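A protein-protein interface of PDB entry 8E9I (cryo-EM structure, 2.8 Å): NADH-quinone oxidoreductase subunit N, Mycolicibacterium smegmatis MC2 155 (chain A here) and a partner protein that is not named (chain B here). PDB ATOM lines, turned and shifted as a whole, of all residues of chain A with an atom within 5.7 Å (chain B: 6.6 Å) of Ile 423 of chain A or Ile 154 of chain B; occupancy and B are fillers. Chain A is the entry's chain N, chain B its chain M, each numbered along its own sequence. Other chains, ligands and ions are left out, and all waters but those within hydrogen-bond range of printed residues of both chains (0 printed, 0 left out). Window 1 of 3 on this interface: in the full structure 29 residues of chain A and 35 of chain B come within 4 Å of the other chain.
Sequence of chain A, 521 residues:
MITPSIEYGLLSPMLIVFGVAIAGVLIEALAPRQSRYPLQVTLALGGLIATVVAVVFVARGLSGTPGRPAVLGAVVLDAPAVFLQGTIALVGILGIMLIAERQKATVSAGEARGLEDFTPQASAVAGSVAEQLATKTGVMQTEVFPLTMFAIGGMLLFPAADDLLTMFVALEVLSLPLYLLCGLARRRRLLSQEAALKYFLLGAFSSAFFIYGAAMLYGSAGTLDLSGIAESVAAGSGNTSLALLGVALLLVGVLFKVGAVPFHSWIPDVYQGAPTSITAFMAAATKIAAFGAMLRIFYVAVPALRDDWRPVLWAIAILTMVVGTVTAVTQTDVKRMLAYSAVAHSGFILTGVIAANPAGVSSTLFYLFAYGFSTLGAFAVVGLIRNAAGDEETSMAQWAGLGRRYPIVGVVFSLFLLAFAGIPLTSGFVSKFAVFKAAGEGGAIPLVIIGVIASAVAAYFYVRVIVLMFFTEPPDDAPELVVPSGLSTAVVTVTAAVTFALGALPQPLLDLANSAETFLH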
ATOM      1  N   LEU A 418      18.599 -19.792 -24.064  1.00  0.00           N
ATOM      2  CA  LEU A 418      18.534 -18.820 -22.982  1.00  0.00           C
ATOM      3  C   LEU A 418      17.333 -17.905 -23.149  1.00  0.00           C
ATOM      4  O   LEU A 418      16.669 -17.569 -22.164  1.00  0.00           O
ATOM      5  CB  LEU A 418      19.824 -18.005 -22.936  1.00  0.00           C
ATOM      6  CG  LEU A 418      21.096 -18.804 -22.643  1.00  0.00           C
ATOM      7  CD1 LEU A 418      22.320 -18.055 -23.133  1.00  0.00           C
ATOM      8  CD2 LEU A 418      21.221 -19.099 -21.166  1.00  0.00           C
ATOM      9  N   ALA A 419      17.033 -17.503 -24.383  1.00  0.00           N
ATOM     10  CA  ALA A 419      15.845 -16.696 -24.618  1.00  0.00           C
ATOM     11  C   ALA A 419      14.587 -17.445 -24.204  1.00  0.00           C
ATOM     12  O   ALA A 419      13.719 -16.885 -23.529  1.00  0.00           O
ATOM     13  CB  ALA A 419      15.771 -16.289 -26.087  1.00  0.00           C
ATOM     14  N   ALA A 421      14.387 -19.772 -21.956  1.00  0.00           N
ATOM     15  CA  ALA A 421      14.411 -19.743 -20.499  1.00  0.00           C
ATOM     16  C   ALA A 421      14.116 -18.350 -19.970  1.00  0.00           C
ATOM     17  O   ALA A 421      13.660 -18.201 -18.833  1.00  0.00           O
ATOM     18  CB  ALA A 421      15.767 -20.223 -19.986  1.00  0.00           C
ATOM     19  N   GLY A 422      14.369 -17.323 -20.772  1.00  0.00           N
ATOM     20  CA  GLY A 422      14.105 -15.970 -20.339  1.00  0.00           C
ATOM     21  C   GLY A 422      15.214 -15.350 -19.531  1.00  0.00           C
ATOM     22  O   GLY A 422      14.943 -14.542 -18.639  1.00  0.00           O
ATOM     23  N   ILE A 423      16.460 -15.713 -19.802  1.00  0.00           N
ATOM     24  CA  ILE A 423      17.572 -15.048 -19.115  1.00  0.00           C
ATOM     25  C   ILE A 423      17.691 -13.624 -19.641  1.00  0.00           C
ATOM     26  O   ILE A 423      17.474 -13.396 -20.844  1.00  0.00           O
ATOM     27  CB  ILE A 423      18.877 -15.818 -19.322  1.00  0.00           C
ATOM     28  CG1 ILE A 423      18.679 -17.323 -19.122  1.00  0.00           C
ATOM     29  CG2 ILE A 423      19.929 -15.307 -18.364  1.00  0.00           C
ATOM     30  CD1 ILE A 423      18.092 -17.699 -17.791  1.00  0.00           C
ATOM     31  N   PRO A 424      18.015 -12.644 -18.807  1.00  0.00           N
ATOM     32  CA  PRO A 424      18.105 -11.264 -19.301  1.00  0.00           C
ATOM     33  C   PRO A 424      19.092 -11.089 -20.444  1.00  0.00           C
ATOM     34  O   PRO A 424      19.892 -11.983 -20.727  1.00  0.00           O
ATOM     35  CB  PRO A 424      18.531 -10.488 -18.054  1.00  0.00           C
ATOM     36  CG  PRO A 424      17.969 -11.268 -16.935  1.00  0.00           C
ATOM     37  CD  PRO A 424      18.095 -12.700 -17.339  1.00  0.00           C
ATOM     38  N   LEU A 425      19.013  -9.939 -21.116  1.00  0.00           N
ATOM     39  CA  LEU A 425      19.803  -9.631 -22.307  1.00  0.00           C
ATOM     40  C   LEU A 425      19.304 -10.395 -23.528  1.00  0.00           C
ATOM     41  O   LEU A 425      19.818 -10.203 -24.633  1.00  0.00           O
ATOM     42  CB  LEU A 425      21.290  -9.916 -22.083  1.00  0.00           C
ATOM     43  CG  LEU A 425      21.965  -9.158 -20.942  1.00  0.00           C
ATOM     44  CD1 LEU A 425      23.433  -9.503 -20.881  1.00  0.00           C
ATOM     45  CD2 LEU A 425      21.790  -7.663 -21.122  1.00  0.00           C
ATOM     46  N   THR A 426      18.306 -11.252 -23.346  1.00  0.00           N
ATOM     47  CA  THR A 426      17.656 -11.905 -24.467  1.00  0.00           C
ATOM     48  C   THR A 426      16.213 -11.444 -24.560  1.00  0.00           C
ATOM     49  O   THR A 426      15.566 -11.155 -23.551  1.00  0.00           O
ATOM     50  CB  THR A 426      17.689 -13.420 -24.309  1.00  0.00           C
ATOM     51  OG1 THR A 426      16.708 -13.814 -23.345  1.00  0.00           O
ATOM     52  CG2 THR A 426      19.056 -13.878 -23.849  1.00  0.00           C
ATOM     53  N   SER A 427      15.704 -11.380 -25.787  1.00  0.00           N
ATOM     54  CA  SER A 427      14.324 -10.953 -25.968  1.00  0.00           C
ATOM     55  C   SER A 427      13.377 -11.809 -25.149  1.00  0.00           C
ATOM     56  O   SER A 427      12.323 -11.331 -24.722  1.00  0.00           O
ATOM     57  CB  SER A 427      13.938 -11.015 -27.443  1.00  0.00           C
ATOM     58  OG  SER A 427      14.074 -12.333 -27.935  1.00  0.00           O
ATOM     59  N   GLY A 428      13.731 -13.071 -24.915  1.00  0.00           N
ATOM     60  CA  GLY A 428      12.887 -13.930 -24.110  1.00  0.00           C
ATOM     61  C   GLY A 428      12.654 -13.409 -22.711  1.00  0.00           C
ATOM     62  O   GLY A 428      11.528 -13.492 -22.207  1.00  0.00           O
ATOM     63  N   PHE A 429      13.690 -12.874 -22.062  1.00  0.00           N
ATOM     64  CA  PHE A 429      13.469 -12.229 -20.776  1.00  0.00           C
ATOM     65  C   PHE A 429      12.456 -11.107 -20.912  1.00  0.00           C
ATOM     66  O   PHE A 429      11.314 -11.240 -20.474  1.00  0.00           O
ATOM     67  CB  PHE A 429      14.770 -11.683 -20.209  1.00  0.00           C
ATOM     68  CG  PHE A 429      14.562 -10.793 -19.028  1.00  0.00           C
ATOM     69  CD1 PHE A 429      14.057 -11.302 -17.850  1.00  0.00           C
ATOM     70  CD2 PHE A 429      14.834  -9.442 -19.105  1.00  0.00           C
ATOM     71  CE1 PHE A 429      13.850 -10.487 -16.764  1.00  0.00           C
ATOM     72  CE2 PHE A 429      14.628  -8.622 -18.021  1.00  0.00           C
ATOM     73  CZ  PHE A 429      14.134  -9.146 -16.850  1.00  0.00           C
ATOM     74  N   ALA A 459      14.294 -23.977 -16.924  1.00  0.00           N
ATOM     75  CA  ALA A 459      15.687 -23.621 -17.138  1.00  0.00           C
ATOM     76  C   ALA A 459      16.564 -24.858 -17.110  1.00  0.00           C
ATOM     77  O   ALA A 459      17.589 -24.915 -17.792  1.00  0.00           O
ATOM     78  CB  ALA A 459      16.142 -22.620 -16.080  1.00  0.00           C
ATOM     79  N   LEU B 125      34.830 -14.695 -21.648  1.00  0.00           N
ATOM     80  CA  LEU B 125      33.867 -14.961 -20.590  1.00  0.00           C
ATOM     81  C   LEU B 125      34.277 -14.262 -19.306  1.00  0.00           C
ATOM     82  O   LEU B 125      33.436 -13.682 -18.610  1.00  0.00           O
ATOM     83  CB  LEU B 125      33.737 -16.466 -20.362  1.00  0.00           C
ATOM     84  CG  LEU B 125      33.072 -17.278 -21.471  1.00  0.00           C
ATOM     85  CD1 LEU B 125      33.261 -18.752 -21.203  1.00  0.00           C
ATOM     86  CD2 LEU B 125      31.604 -16.944 -21.584  1.00  0.00           C
ATOM     87  N   VAL B 129      32.025 -11.402 -17.514  1.00  0.00           N
ATOM     88  CA  VAL B 129      31.649 -11.478 -16.107  1.00  0.00           C
ATOM     89  C   VAL B 129      32.054 -10.201 -15.392  1.00  0.00           C
ATOM     90  O   VAL B 129      31.272  -9.619 -14.632  1.00  0.00           O
ATOM     91  CB  VAL B 129      32.287 -12.707 -15.441  1.00  0.00           C
ATOM     92  CG1 VAL B 129      32.225 -12.568 -13.934  1.00  0.00           C
ATOM     93  CG2 VAL B 129      31.591 -13.968 -15.879  1.00  0.00           C
ATOM     94  N   MET B 132      29.744  -7.273 -16.500  1.00  0.00           N
ATOM     95  CA  MET B 132      28.368  -7.415 -16.049  1.00  0.00           C
ATOM     96  C   MET B 132      28.265  -7.236 -14.543  1.00  0.00           C
ATOM     97  O   MET B 132      27.297  -6.644 -14.050  1.00  0.00           O
ATOM     98  CB  MET B 132      27.855  -8.779 -16.493  1.00  0.00           C
ATOM     99  CG  MET B 132      27.751  -8.876 -18.004  1.00  0.00           C
ATOM    100  SD  MET B 132      27.247 -10.484 -18.634  1.00  0.00           S
ATOM    101  CE  MET B 132      25.543 -10.530 -18.128  1.00  0.00           C
ATOM    102  N   VAL B 147      18.555  -7.272 -14.273  1.00  0.00           N
ATOM    103  CA  VAL B 147      19.009  -7.754 -15.571  1.00  0.00           C
ATOM    104  C   VAL B 147      20.442  -8.250 -15.472  1.00  0.00           C
ATOM    105  O   VAL B 147      20.736  -9.418 -15.746  1.00  0.00           O
ATOM    106  CB  VAL B 147      18.869  -6.640 -16.625  1.00  0.00           C
ATOM    107  CG1 VAL B 147      19.504  -7.033 -17.946  1.00  0.00           C
ATOM    108  CG2 VAL B 147      17.410  -6.324 -16.852  1.00  0.00           C
ATOM    109  N   GLU B 150      21.189 -11.195 -12.861  1.00  0.00           N
ATOM    110  CA  GLU B 150      20.784 -12.508 -13.330  1.00  0.00           C
ATOM    111  C   GLU B 150      21.630 -12.963 -14.507  1.00  0.00           C
ATOM    112  O   GLU B 150      22.047 -14.123 -14.560  1.00  0.00           O
ATOM    113  CB  GLU B 150      19.307 -12.485 -13.725  1.00  0.00           C
ATOM    114  N   ALA B 151      21.908 -12.063 -15.447  1.00  0.00           N
ATOM    115  CA  ALA B 151      22.590 -12.468 -16.669  1.00  0.00           C
ATOM    116  C   ALA B 151      24.019 -12.917 -16.391  1.00  0.00           C
ATOM    117  O   ALA B 151      24.490 -13.895 -16.981  1.00  0.00           O
ATOM    118  CB  ALA B 151      22.559 -11.324 -17.675  1.00  0.00           C
ATOM    119  N   MET B 152      24.726 -12.235 -15.484  1.00  0.00           N
ATOM    120  CA  MET B 152      26.112 -12.611 -15.229  1.00  0.00           C
ATOM    121  C   MET B 152      26.239 -14.059 -14.788  1.00  0.00           C
ATOM    122  O   MET B 152      27.356 -14.581 -14.727  1.00  0.00           O
ATOM    123  CB  MET B 152      26.737 -11.709 -14.167  1.00  0.00           C
ATOM    124  CG  MET B 152      26.122 -11.850 -12.794  1.00  0.00           C
ATOM    125  SD  MET B 152      26.856 -10.736 -11.590  1.00  0.00           S
ATOM    126  CE  MET B 152      25.911 -11.147 -10.128  1.00  0.00           C
ATOM    127  N   LEU B 153      25.124 -14.716 -14.471  1.00  0.00           N
ATOM    128  CA  LEU B 153      25.157 -16.141 -14.177  1.00  0.00           C
ATOM    129  C   LEU B 153      25.552 -16.963 -15.396  1.00  0.00           C
ATOM    130  O   LEU B 153      26.140 -18.039 -15.252  1.00  0.00           O
ATOM    131  CB  LEU B 153      23.789 -16.592 -13.669  1.00  0.00           C
ATOM    132  CG  LEU B 153      23.300 -15.912 -12.391  1.00  0.00           C
ATOM    133  CD1 LEU B 153      21.865 -16.302 -12.085  1.00  0.00           C
ATOM    134  CD2 LEU B 153      24.203 -16.239 -11.217  1.00  0.00           C
ATOM    135  N   ILE B 154      25.237 -16.486 -16.597  1.00  0.00           N
ATOM    136  CA  ILE B 154      25.406 -17.286 -17.808  1.00  0.00           C
ATOM    137  C   ILE B 154      26.872 -17.335 -18.212  1.00  0.00           C
ATOM    138  O   ILE B 154      27.400 -18.424 -18.484  1.00  0.00           O
ATOM    139  CB  ILE B 154      24.543 -16.746 -18.958  1.00  0.00           C
ATOM    140  CG1 ILE B 154      23.062 -16.888 -18.622  1.00  0.00           C
ATOM    141  CG2 ILE B 154      24.873 -17.478 -20.245  1.00  0.00           C
ATOM    142  CD1 ILE B 154      22.622 -18.299 -18.307  1.00  0.00           C
ATOM    143  N   PRO B 155      27.569 -16.202 -18.291  1.00  0.00           N
ATOM    144  CA  PRO B 155      28.998 -16.283 -18.607  1.00  0.00           C
ATOM    145  C   PRO B 155      29.749 -17.170 -17.639  1.00  0.00           C
ATOM    146  O   PRO B 155      30.613 -17.947 -18.055  1.00  0.00           O
ATOM    147  CB  PRO B 155      29.453 -14.823 -18.520  1.00  0.00           C
ATOM    148  CG  PRO B 155      28.233 -14.036 -18.765  1.00  0.00           C
ATOM    149  CD  PRO B 155      27.129 -14.807 -18.132  1.00  0.00           C
ATOM    150  N   MET B 156      29.415 -17.110 -16.352  1.00  0.00           N
ATOM    151  CA  MET B 156      30.086 -17.979 -15.395  1.00  0.00           C
ATOM    152  C   MET B 156      29.581 -19.405 -15.487  1.00  0.00           C
ATOM    153  O   MET B 156      30.319 -20.344 -15.182  1.00  0.00           O
ATOM    154  CB  MET B 156      29.919 -17.445 -13.982  1.00  0.00           C
ATOM    155  CG  MET B 156      30.594 -18.306 -12.922  1.00  0.00           C
ATOM    156  SD  MET B 156      32.388 -18.252 -12.974  1.00  0.00           S
ATOM    157  CE  MET B 156      32.709 -16.608 -12.361  1.00  0.00           C
ATOM    158  N   TYR B 157      28.332 -19.602 -15.888  1.00  0.00           N
ATOM    159  CA  TYR B 157      27.874 -20.965 -16.113  1.00  0.00           C
ATOM    160  C   TYR B 157      28.713 -21.626 -17.197  1.00  0.00           C
ATOM    161  O   TYR B 157      29.162 -22.769 -17.047  1.00  0.00           O
ATOM    162  CB  TYR B 157      26.392 -20.958 -16.476  1.00  0.00           C
ATOM    163  CG  TYR B 157      25.950 -22.120 -17.316  1.00  0.00           C
ATOM    164  CD1 TYR B 157      25.717 -23.360 -16.750  1.00  0.00           C
ATOM    165  CD2 TYR B 157      25.727 -21.966 -18.672  1.00  0.00           C
ATOM    166  CE1 TYR B 157      25.302 -24.417 -17.513  1.00  0.00           C
ATOM    167  CE2 TYR B 157      25.310 -23.015 -19.442  1.00  0.00           C
ATOM    168  CZ  TYR B 157      25.097 -24.238 -18.860  1.00  0.00           C
ATOM    169  OH  TYR B 157      24.684 -25.287 -19.639  1.00  0.00           O
ATOM    170  N   PHE B 158      28.975 -20.898 -18.280  1.00  0.00           N
ATOM    171  CA  PHE B 158      29.877 -21.408 -19.305  1.00  0.00           C
ATOM    172  C   PHE B 158      31.286 -21.582 -18.758  1.00  0.00           C
ATOM    173  O   PHE B 158      31.931 -22.611 -18.988  1.00  0.00           O
ATOM    174  CB  PHE B 158      29.894 -20.460 -20.500  1.00  0.00           C
ATOM    175  CG  PHE B 158      28.706 -20.601 -21.393  1.00  0.00           C
ATOM    176  CD1 PHE B 158      28.568 -21.699 -22.213  1.00  0.00           C
ATOM    177  CD2 PHE B 158      27.729 -19.630 -21.416  1.00  0.00           C
ATOM    178  CE1 PHE B 158      27.478 -21.828 -23.031  1.00  0.00           C
ATOM    179  CE2 PHE B 158      26.641 -19.752 -22.235  1.00  0.00           C
ATOM    180  CZ  PHE B 158      26.515 -20.853 -23.045  1.00  0.00           C
ATOM    181  N   LEU B 159      31.783 -20.585 -18.024  1.00  0.00           N
ATOM    182  CA  LEU B 159      33.150 -20.631 -17.527  1.00  0.00           C
ATOM    183  C   LEU B 159      33.374 -21.804 -16.585  1.00  0.00           C
ATOM    184  O   LEU B 159      34.478 -22.352 -16.551  1.00  0.00           O
ATOM    185  CB  LEU B 159      33.476 -19.308 -16.832  1.00  0.00           C
ATOM    186  CG  LEU B 159      34.941 -18.912 -16.656  1.00  0.00           C
ATOM    187  CD1 LEU B 159      35.668 -18.874 -17.982  1.00  0.00           C
ATOM    188  CD2 LEU B 159      35.022 -17.557 -15.972  1.00  0.00           C
ATOM    189  N   PHE B 175      24.984 -24.957 -10.005  1.00  0.00           N
ATOM    190  CA  PHE B 175      25.211 -23.534  -9.787  1.00  0.00           C
ATOM    191  C   PHE B 175      24.168 -22.699 -10.512  1.00  0.00           C
ATOM    192  O   PHE B 175      23.468 -21.877  -9.905  1.00  0.00           O
ATOM    193  CB  PHE B 175      26.620 -23.168 -10.260  1.00  0.00           C
ATOM    194  CG  PHE B 175      26.775 -21.733 -10.664  1.00  0.00           C
ATOM    195  CD1 PHE B 175      27.120 -20.772  -9.737  1.00  0.00           C
ATOM    196  CD2 PHE B 175      26.583 -21.347 -11.975  1.00  0.00           C
ATOM    197  CE1 PHE B 175      27.261 -19.455 -10.106  1.00  0.00           C
ATOM    198  CE2 PHE B 175      26.722 -20.034 -12.347  1.00  0.00           C
ATOM    199  CZ  PHE B 175      27.063 -19.087 -11.412  1.00  0.00           C
ATOM    200  N   LEU B 176      24.033 -22.918 -11.818  1.00  0.00           N
ATOM    201  CA  LEU B 176      23.143 -22.082 -12.607  1.00  0.00           C
ATOM    202  C   LEU B 176      21.706 -22.232 -12.141  1.00  0.00           C
ATOM    203  O   LEU B 176      20.969 -21.252 -12.073  1.00  0.00           O
ATOM    204  CB  LEU B 176      23.261 -22.424 -14.088  1.00  0.00           C
ATOM    205  CG  LEU B 176      22.324 -21.624 -14.995  1.00  0.00           C
ATOM    206  CD1 LEU B 176      22.566 -20.132 -14.845  1.00  0.00           C
ATOM    207  CD2 LEU B 176      22.493 -22.043 -16.432  1.00  0.00           C
ATOM    208  N   LEU B 180      19.660 -19.251 -10.619  1.00  0.00           N
ATOM    209  CA  LEU B 180      18.617 -18.763 -11.501  1.00  0.00           C
ATOM    210  C   LEU B 180      17.246 -18.929 -10.875  1.00  0.00           C
ATOM    211  O   LEU B 180      16.358 -18.112 -11.114  1.00  0.00           O
ATOM    212  CB  LEU B 180      18.693 -19.500 -12.834  1.00  0.00           C
ATOM    213  CG  LEU B 180      17.762 -19.018 -13.941  1.00  0.00           C
ATOM    214  CD1 LEU B 180      18.030 -17.564 -14.266  1.00  0.00           C
ATOM    215  CD2 LEU B 180      17.932 -19.885 -15.170  1.00  0.00           C
ATOM    216  N   LEU B 184      14.853 -15.837 -10.403  1.00  0.00           N
ATOM    217  CA  LEU B 184      13.474 -15.823 -10.867  1.00  0.00           C
ATOM    218  C   LEU B 184      12.520 -15.496  -9.728  1.00  0.00           C
ATOM    219  O   LEU B 184      11.504 -14.822  -9.931  1.00  0.00           O
ATOM    220  CB  LEU B 184      13.133 -17.167 -11.503  1.00  0.00           C
ATOM    221  CG  LEU B 184      13.837 -17.453 -12.826  1.00  0.00           C
ATOM    222  CD1 LEU B 184      13.742 -18.924 -13.144  1.00  0.00           C
ATOM    223  CD2 LEU B 184      13.235 -16.619 -13.943  1.00  0.00           C
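N of Ile 423 of chain A lies within hydrogen-bond range of O of Leu 418 of chain A.
The backbone carbonyl oxygen of Ile 423 of chain A sits at hydrogen-bond distance from the side-chain hydroxyl of Thr 426 of chain A (2.6 Å).
OG1 of Thr 426 of chain A sits at hydrogen-bond distance from N of Phe 429 of chain A.
Leu 418 of chain A touches Ile 154 of chain B.
Ile 154 of chain B touches Ile 423 of chain A.
CD2 of Leu 180 of chain B touches CD1 of Ile 423 of chain A, 3.4 Å away.
Pro 424 of chain A touches Val 147 of chain B.
Glu 150 of chain B touches Pro 424 of chain A (CB to CG, 3.7 Å).
Leu 425 of chain A touches Met 132 of chain B.
Leu 425 of chain A touches Val 147 of chain B.
Ala 151 of chain B touches Leu 425 of chain A (CB to CD1, 3.8 Å).
Val 147 of chain B touches Phe 429 of chain A (CG2 to CE2, 3.8 Å).
Leu 180 of chain B touches Ala 459 of chain A (CD2 to CB, 3.4 Å).
Hydrophobic or aromatic side chains of chain A within 4 Å of the printed part of chain B: Leu 418, Ile 423, Pro 424, Leu 425, Phe 429 and Ala 459.
Hydrophobic or aromatic side chains of chain B within 4 Å of the printed part of chain A: Met 132, Val 147, Ala 151, Ile 154 and Leu 180.
Among the printed residues, 10 pairs touch across the chains.
Of chain B, only Ile 154 (3.5 Å) and Leu 180 (3.4 Å) come within 4 Å of Ile 423 of chain A.
Of chain A, only Leu 418 (3.3 Å) and Ile 423 (3.5 Å) come within 4 Å of Ile 154 of chain B.
Of the printed residues of chain A, Met 132 of chain B touches Leu 425.
Of the printed residues of chain B, Phe 429 of chain A touches Val 147.
Printed residues of chain B within 4 Å of Pro 424 of chain A: Val 147 (3.4 Å) and Glu 150 (3.7 Å).
Of the printed residues of chain A, Val 147 of chain B touches Pro 424, Leu 425 and Phe 429.
Phe 175 of chain B touches none of the printed residues of chain A.
Leu 125 of chain B touches none of the printed residues of chain A.
The nearest printed residue of chain A that does not touch Val 147 of chain B is Ile 423 of chain A (6.5 Å).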
